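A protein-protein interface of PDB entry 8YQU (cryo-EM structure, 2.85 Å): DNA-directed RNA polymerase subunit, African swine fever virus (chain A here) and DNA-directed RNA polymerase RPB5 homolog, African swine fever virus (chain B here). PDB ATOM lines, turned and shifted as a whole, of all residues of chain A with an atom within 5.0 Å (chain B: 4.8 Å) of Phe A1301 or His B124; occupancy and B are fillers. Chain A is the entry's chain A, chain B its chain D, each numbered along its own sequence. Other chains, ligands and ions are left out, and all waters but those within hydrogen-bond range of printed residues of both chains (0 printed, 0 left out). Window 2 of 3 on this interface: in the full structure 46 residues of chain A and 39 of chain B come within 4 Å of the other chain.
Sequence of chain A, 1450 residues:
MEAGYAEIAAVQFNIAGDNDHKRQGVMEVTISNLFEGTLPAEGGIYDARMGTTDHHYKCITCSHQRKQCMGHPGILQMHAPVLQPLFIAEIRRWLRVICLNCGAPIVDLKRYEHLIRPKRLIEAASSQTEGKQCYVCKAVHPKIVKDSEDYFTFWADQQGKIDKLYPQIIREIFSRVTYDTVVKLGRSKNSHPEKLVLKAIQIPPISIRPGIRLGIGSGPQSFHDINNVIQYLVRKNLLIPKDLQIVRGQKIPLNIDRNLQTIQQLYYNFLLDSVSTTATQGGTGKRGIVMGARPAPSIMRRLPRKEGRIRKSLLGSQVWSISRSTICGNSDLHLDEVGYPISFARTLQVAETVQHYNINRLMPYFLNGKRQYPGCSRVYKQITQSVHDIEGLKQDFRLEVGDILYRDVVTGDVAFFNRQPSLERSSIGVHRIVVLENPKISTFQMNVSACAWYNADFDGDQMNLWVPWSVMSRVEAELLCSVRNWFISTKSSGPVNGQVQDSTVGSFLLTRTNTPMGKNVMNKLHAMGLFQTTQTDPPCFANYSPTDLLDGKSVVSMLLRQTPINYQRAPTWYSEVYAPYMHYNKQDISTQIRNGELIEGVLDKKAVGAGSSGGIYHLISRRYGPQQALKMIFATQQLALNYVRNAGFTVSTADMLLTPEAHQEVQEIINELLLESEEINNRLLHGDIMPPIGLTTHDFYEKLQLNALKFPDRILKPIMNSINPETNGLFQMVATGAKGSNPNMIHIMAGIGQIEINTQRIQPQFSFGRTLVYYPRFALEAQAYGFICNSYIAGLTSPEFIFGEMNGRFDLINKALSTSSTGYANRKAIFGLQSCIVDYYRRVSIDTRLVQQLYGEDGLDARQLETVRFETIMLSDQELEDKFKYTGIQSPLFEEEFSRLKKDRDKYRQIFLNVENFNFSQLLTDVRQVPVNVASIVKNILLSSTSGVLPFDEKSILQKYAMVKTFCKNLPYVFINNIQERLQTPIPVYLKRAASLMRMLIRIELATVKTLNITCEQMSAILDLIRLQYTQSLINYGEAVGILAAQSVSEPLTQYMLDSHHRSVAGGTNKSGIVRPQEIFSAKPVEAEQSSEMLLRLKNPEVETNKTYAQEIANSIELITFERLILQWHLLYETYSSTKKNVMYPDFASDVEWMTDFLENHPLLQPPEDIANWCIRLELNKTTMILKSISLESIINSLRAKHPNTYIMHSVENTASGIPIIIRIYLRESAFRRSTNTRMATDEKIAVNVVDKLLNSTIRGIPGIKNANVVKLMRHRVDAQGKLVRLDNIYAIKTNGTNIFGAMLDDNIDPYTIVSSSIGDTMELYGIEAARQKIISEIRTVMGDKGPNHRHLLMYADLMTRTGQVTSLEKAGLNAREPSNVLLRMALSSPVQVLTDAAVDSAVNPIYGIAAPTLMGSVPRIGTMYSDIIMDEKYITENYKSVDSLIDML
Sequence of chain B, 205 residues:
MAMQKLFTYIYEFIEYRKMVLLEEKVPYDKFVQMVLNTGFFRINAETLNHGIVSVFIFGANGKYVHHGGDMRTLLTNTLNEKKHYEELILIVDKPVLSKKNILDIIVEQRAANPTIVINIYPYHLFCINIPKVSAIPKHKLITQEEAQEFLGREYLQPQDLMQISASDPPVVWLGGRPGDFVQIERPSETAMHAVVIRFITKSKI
SG of Cys B127 lies within hydrogen-bond range of O of Tyr B123.
Among the printed residues, pairs that only touch across the chains: Phe A1301 with Cys B127 (3.4 Å), Glu A1324 with Lys B94 (3.4 Å), Phe A1301 with His B124 (3.5 Å), Met A1304 with Cys B127 (3.6 Å), Leu A1305 with Ala B2 (3.6 Å), Glu A1324 with His B124 (3.6 Å) and Leu A1325 with His B124 (3.9 Å).
His B124 touches three residues of chain A. Of the printed residues of chain B, Leu A1325 touches His B124. Printed residues of chain B within 4 Å of Leu A1305: Ala B2. Printed residues of chain A within 4 Å of Lys B94: Glu A1324 (3.4 Å). Printed residues of chain A within 4 Å of Cys B127: Phe A1301 and Met A1304. Printed residues of chain B within 4 Å of Glu A1324: Lys B94 (3.4 Å) and His B124 (3.6 Å). The nearest residue of chain B that does not touch Phe A1301 is Ala B2 (4.3 Å). The nearest residue of chain A that does not touch His B124 is Met A1304 (4.04 Å). The nearest printed residue of chain A that does not touch Lys B94 is Phe A1301 (6.5 Å).
Of the 9 printed residues of chain A, 5 touch a printed residue of chain B. Hydrophobic or aromatic side chains of chain A within 4 Å of the printed part of chain B: Phe A1301, Met A1304, Leu A1305 and Leu A1325. Among the printed residues, 7 pairs touch across the chains. Among the printed residues, no Asp or Glu carboxylate lies within 4 Å of a Lys or Arg side-chain nitrogen of the other chain.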
ATOM      1  N   ASN A1299       5.790 -13.651  32.381  1.00  0.00           N
ATOM      2  CA  ASN A1299       6.789 -13.655  31.313  1.00  0.00           C
ATOM      3  C   ASN A1299       6.223 -12.815  30.172  1.00  0.00           C
ATOM      4  O   ASN A1299       5.501 -13.336  29.318  1.00  0.00           O
ATOM      5  CB  ASN A1299       7.110 -15.073  30.860  1.00  0.00           C
ATOM      6  CG  ASN A1299       8.363 -15.144  30.013  1.00  0.00           C
ATOM      7  OD1 ASN A1299       9.039 -14.139  29.798  1.00  0.00           O
ATOM      8  ND2 ASN A1299       8.680 -16.337  29.524  1.00  0.00           N
ATOM      9  N   ILE A1300       6.554 -11.522  30.166  1.00  0.00           N
ATOM     10  CA  ILE A1300       6.042 -10.639  29.122  1.00  0.00           C
ATOM     11  C   ILE A1300       6.609 -11.033  27.766  1.00  0.00           C
ATOM     12  O   ILE A1300       5.886 -11.076  26.765  1.00  0.00           O
ATOM     13  CB  ILE A1300       6.348  -9.168  29.456  1.00  0.00           C
ATOM     14  CG1 ILE A1300       5.690  -8.763  30.773  1.00  0.00           C
ATOM     15  CG2 ILE A1300       5.871  -8.256  28.336  1.00  0.00           C
ATOM     16  CD1 ILE A1300       6.096  -7.389  31.248  1.00  0.00           C
ATOM     17  N   PHE A1301       7.909 -11.332  27.710  1.00  0.00           N
ATOM     18  CA  PHE A1301       8.532 -11.674  26.436  1.00  0.00           C
ATOM     19  C   PHE A1301       8.054 -13.028  25.927  1.00  0.00           C
ATOM     20  O   PHE A1301       7.961 -13.242  24.714  1.00  0.00           O
ATOM     21  CB  PHE A1301      10.054 -11.656  26.574  1.00  0.00           C
ATOM     22  CG  PHE A1301      10.778 -11.905  25.285  1.00  0.00           C
ATOM     23  CD1 PHE A1301      10.397 -11.248  24.129  1.00  0.00           C
ATOM     24  CD2 PHE A1301      11.844 -12.786  25.228  1.00  0.00           C
ATOM     25  CE1 PHE A1301      11.058 -11.469  22.941  1.00  0.00           C
ATOM     26  CE2 PHE A1301      12.510 -13.010  24.040  1.00  0.00           C
ATOM     27  CZ  PHE A1301      12.116 -12.350  22.895  1.00  0.00           C
ATOM     28  N   GLY A1302       7.759 -13.958  26.838  1.00  0.00           N
ATOM     29  CA  GLY A1302       7.233 -15.246  26.414  1.00  0.00           C
ATOM     30  C   GLY A1302       5.872 -15.131  25.754  1.00  0.00           C
ATOM     31  O   GLY A1302       5.632 -15.723  24.700  1.00  0.00           O
ATOM     32  N   ALA A1303       4.966 -14.363  26.363  1.00  0.00           N
ATOM     33  CA  ALA A1303       3.664 -14.126  25.748  1.00  0.00           C
ATOM     34  C   ALA A1303       3.764 -13.124  24.607  1.00  0.00           C
ATOM     35  O   ALA A1303       2.850 -13.033  23.781  1.00  0.00           O
ATOM     36  CB  ALA A1303       2.669 -13.641  26.799  1.00  0.00           C
ATOM     37  N   MET A1304       4.856 -12.361  24.558  1.00  0.00           N
ATOM     38  CA  MET A1304       5.094 -11.450  23.444  1.00  0.00           C
ATOM     39  C   MET A1304       5.209 -12.200  22.126  1.00  0.00           C
ATOM     40  O   MET A1304       4.693 -11.738  21.102  1.00  0.00           O
ATOM     41  CB  MET A1304       6.373 -10.657  23.698  1.00  0.00           C
ATOM     42  CG  MET A1304       6.667  -9.574  22.692  1.00  0.00           C
ATOM     43  SD  MET A1304       8.215  -8.737  23.081  1.00  0.00           S
ATOM     44  CE  MET A1304       7.765  -7.837  24.560  1.00  0.00           C
ATOM     45  N   LEU A1305       5.882 -13.350  22.135  1.00  0.00           N
ATOM     46  CA  LEU A1305       6.165 -14.100  20.922  1.00  0.00           C
ATOM     47  C   LEU A1305       4.988 -14.948  20.458  1.00  0.00           C
ATOM     48  O   LEU A1305       4.992 -15.409  19.312  1.00  0.00           O
ATOM     49  CB  LEU A1305       7.385 -14.993  21.148  1.00  0.00           C
ATOM     50  CG  LEU A1305       8.678 -14.232  21.448  1.00  0.00           C
ATOM     51  CD1 LEU A1305       9.812 -15.187  21.795  1.00  0.00           C
ATOM     52  CD2 LEU A1305       9.056 -13.324  20.295  1.00  0.00           C
ATOM     53  N   GLU A1324      11.797  -3.891  32.531  1.00  0.00           N
ATOM     54  CA  GLU A1324      12.818  -4.463  31.661  1.00  0.00           C
ATOM     55  C   GLU A1324      12.449  -4.326  30.189  1.00  0.00           C
ATOM     56  O   GLU A1324      13.310  -4.029  29.353  1.00  0.00           O
ATOM     57  CB  GLU A1324      13.041  -5.932  32.023  1.00  0.00           C
ATOM     58  CG  GLU A1324      14.117  -6.619  31.200  1.00  0.00           C
ATOM     59  CD  GLU A1324      14.272  -8.083  31.558  1.00  0.00           C
ATOM     60  OE1 GLU A1324      13.471  -8.586  32.373  1.00  0.00           O
ATOM     61  OE2 GLU A1324      15.197  -8.731  31.024  1.00  0.00           O
ATOM     62  N   LEU A1325      11.177  -4.535  29.850  1.00  0.00           N
ATOM     63  CA  LEU A1325      10.767  -4.636  28.456  1.00  0.00           C
ATOM     64  C   LEU A1325      10.087  -3.386  27.915  1.00  0.00           C
ATOM     65  O   LEU A1325      10.131  -3.160  26.701  1.00  0.00           O
ATOM     66  CB  LEU A1325       9.827  -5.832  28.264  1.00  0.00           C
ATOM     67  CG  LEU A1325      10.465  -7.223  28.195  1.00  0.00           C
ATOM     68  CD1 LEU A1325      10.981  -7.684  29.544  1.00  0.00           C
ATOM     69  CD2 LEU A1325       9.476  -8.224  27.645  1.00  0.00           C
ATOM     70  N   ALA B   2      11.234 -15.698  18.307  1.00  0.00           N
ATOM     71  CA  ALA B   2      11.893 -14.400  18.381  1.00  0.00           C
ATOM     72  C   ALA B   2      12.331 -13.917  17.003  1.00  0.00           C
ATOM     73  O   ALA B   2      12.119 -12.749  16.655  1.00  0.00           O
ATOM     74  CB  ALA B   2      13.090 -14.470  19.329  1.00  0.00           C
ATOM     75  N   LYS B  94      19.542 -12.148  24.945  1.00  0.00           N
ATOM     76  CA  LYS B  94      19.650 -11.536  26.268  1.00  0.00           C
ATOM     77  C   LYS B  94      20.771 -12.117  27.126  1.00  0.00           C
ATOM     78  O   LYS B  94      21.486 -11.323  27.764  1.00  0.00           O
ATOM     79  CB  LYS B  94      18.303 -11.632  26.998  1.00  0.00           C
ATOM     80  CG  LYS B  94      18.259 -10.847  28.301  1.00  0.00           C
ATOM     81  CD  LYS B  94      16.884 -10.902  28.946  1.00  0.00           C
ATOM     82  CE  LYS B  94      16.625 -12.255  29.581  1.00  0.00           C
ATOM     83  NZ  LYS B  94      17.534 -12.508  30.732  1.00  0.00           N
ATOM     84  N   PRO B 122      19.149  -6.419  23.511  1.00  0.00           N
ATOM     85  CA  PRO B 122      18.587  -7.772  23.499  1.00  0.00           C
ATOM     86  C   PRO B 122      17.525  -7.913  22.411  1.00  0.00           C
ATOM     87  O   PRO B 122      17.145  -6.951  21.747  1.00  0.00           O
ATOM     88  CB  PRO B 122      17.980  -7.908  24.896  1.00  0.00           C
ATOM     89  CG  PRO B 122      17.655  -6.514  25.291  1.00  0.00           C
ATOM     90  CD  PRO B 122      18.717  -5.650  24.690  1.00  0.00           C
ATOM     91  N   TYR B 123      17.053  -9.150  22.235  1.00  0.00           N
ATOM     92  CA  TYR B 123      16.007  -9.409  21.249  1.00  0.00           C
ATOM     93  C   TYR B 123      14.696  -8.722  21.614  1.00  0.00           C
ATOM     94  O   TYR B 123      14.024  -8.163  20.741  1.00  0.00           O
ATOM     95  CB  TYR B 123      15.776 -10.913  21.094  1.00  0.00           C
ATOM     96  CG  TYR B 123      16.884 -11.660  20.390  1.00  0.00           C
ATOM     97  CD1 TYR B 123      17.851 -10.985  19.659  1.00  0.00           C
ATOM     98  CD2 TYR B 123      16.948 -13.046  20.440  1.00  0.00           C
ATOM     99  CE1 TYR B 123      18.858 -11.670  19.007  1.00  0.00           C
ATOM    100  CE2 TYR B 123      17.950 -13.737  19.794  1.00  0.00           C
ATOM    101  CZ  TYR B 123      18.902 -13.046  19.079  1.00  0.00           C
ATOM    102  OH  TYR B 123      19.901 -13.735  18.435  1.00  0.00           O
ATOM    103  N   HIS B 124      14.316  -8.749  22.895  1.00  0.00           N
ATOM    104  CA  HIS B 124      12.966  -8.339  23.272  1.00  0.00           C
ATOM    105  C   HIS B 124      12.704  -6.860  23.020  1.00  0.00           C
ATOM    106  O   HIS B 124      11.539  -6.447  23.013  1.00  0.00           O
ATOM    107  CB  HIS B 124      12.692  -8.670  24.741  1.00  0.00           C
ATOM    108  CG  HIS B 124      13.637  -8.019  25.704  1.00  0.00           C
ATOM    109  ND1 HIS B 124      13.591  -6.674  25.998  1.00  0.00           N
ATOM    110  CD2 HIS B 124      14.635  -8.536  26.458  1.00  0.00           C
ATOM    111  CE1 HIS B 124      14.529  -6.387  26.882  1.00  0.00           C
ATOM    112  NE2 HIS B 124      15.176  -7.499  27.179  1.00  0.00           N
ATOM    113  N   LEU B 125      13.746  -6.057  22.813  1.00  0.00           N
ATOM    114  CA  LEU B 125      13.537  -4.641  22.546  1.00  0.00           C
ATOM    115  C   LEU B 125      13.085  -4.386  21.114  1.00  0.00           C
ATOM    116  O   LEU B 125      12.546  -3.310  20.835  1.00  0.00           O
ATOM    117  CB  LEU B 125      14.824  -3.868  22.867  1.00  0.00           C
ATOM    118  CG  LEU B 125      14.858  -2.335  22.898  1.00  0.00           C
ATOM    119  CD1 LEU B 125      15.945  -1.882  23.854  1.00  0.00           C
ATOM    120  CD2 LEU B 125      15.105  -1.728  21.529  1.00  0.00           C
ATOM    121  N   PHE B 126      13.255  -5.356  20.212  1.00  0.00           N
ATOM    122  CA  PHE B 126      12.892  -5.196  18.809  1.00  0.00           C
ATOM    123  C   PHE B 126      11.846  -6.222  18.382  1.00  0.00           C
ATOM    124  O   PHE B 126      11.750  -6.556  17.200  1.00  0.00           O
ATOM    125  CB  PHE B 126      14.122  -5.299  17.908  1.00  0.00           C
ATOM    126  CG  PHE B 126      15.104  -4.180  18.086  1.00  0.00           C
ATOM    127  CD1 PHE B 126      14.994  -3.019  17.341  1.00  0.00           C
ATOM    128  CD2 PHE B 126      16.150  -4.295  18.984  1.00  0.00           C
ATOM    129  CE1 PHE B 126      15.902  -1.991  17.499  1.00  0.00           C
ATOM    130  CE2 PHE B 126      17.061  -3.272  19.145  1.00  0.00           C
ATOM    131  CZ  PHE B 126      16.936  -2.118  18.402  1.00  0.00           C
ATOM    132  N   CYS B 127      11.064  -6.740  19.328  1.00  0.00           N
ATOM    133  CA  CYS B 127      10.044  -7.737  19.030  1.00  0.00           C
ATOM    134  C   CYS B 127       8.636  -7.159  18.968  1.00  0.00           C
ATOM    135  O   CYS B 127       7.695  -7.889  18.640  1.00  0.00           O
ATOM    136  CB  CYS B 127      10.089  -8.866  20.062  1.00  0.00           C
ATOM    137  SG  CYS B 127      11.524  -9.945  19.916  1.00  0.00           S
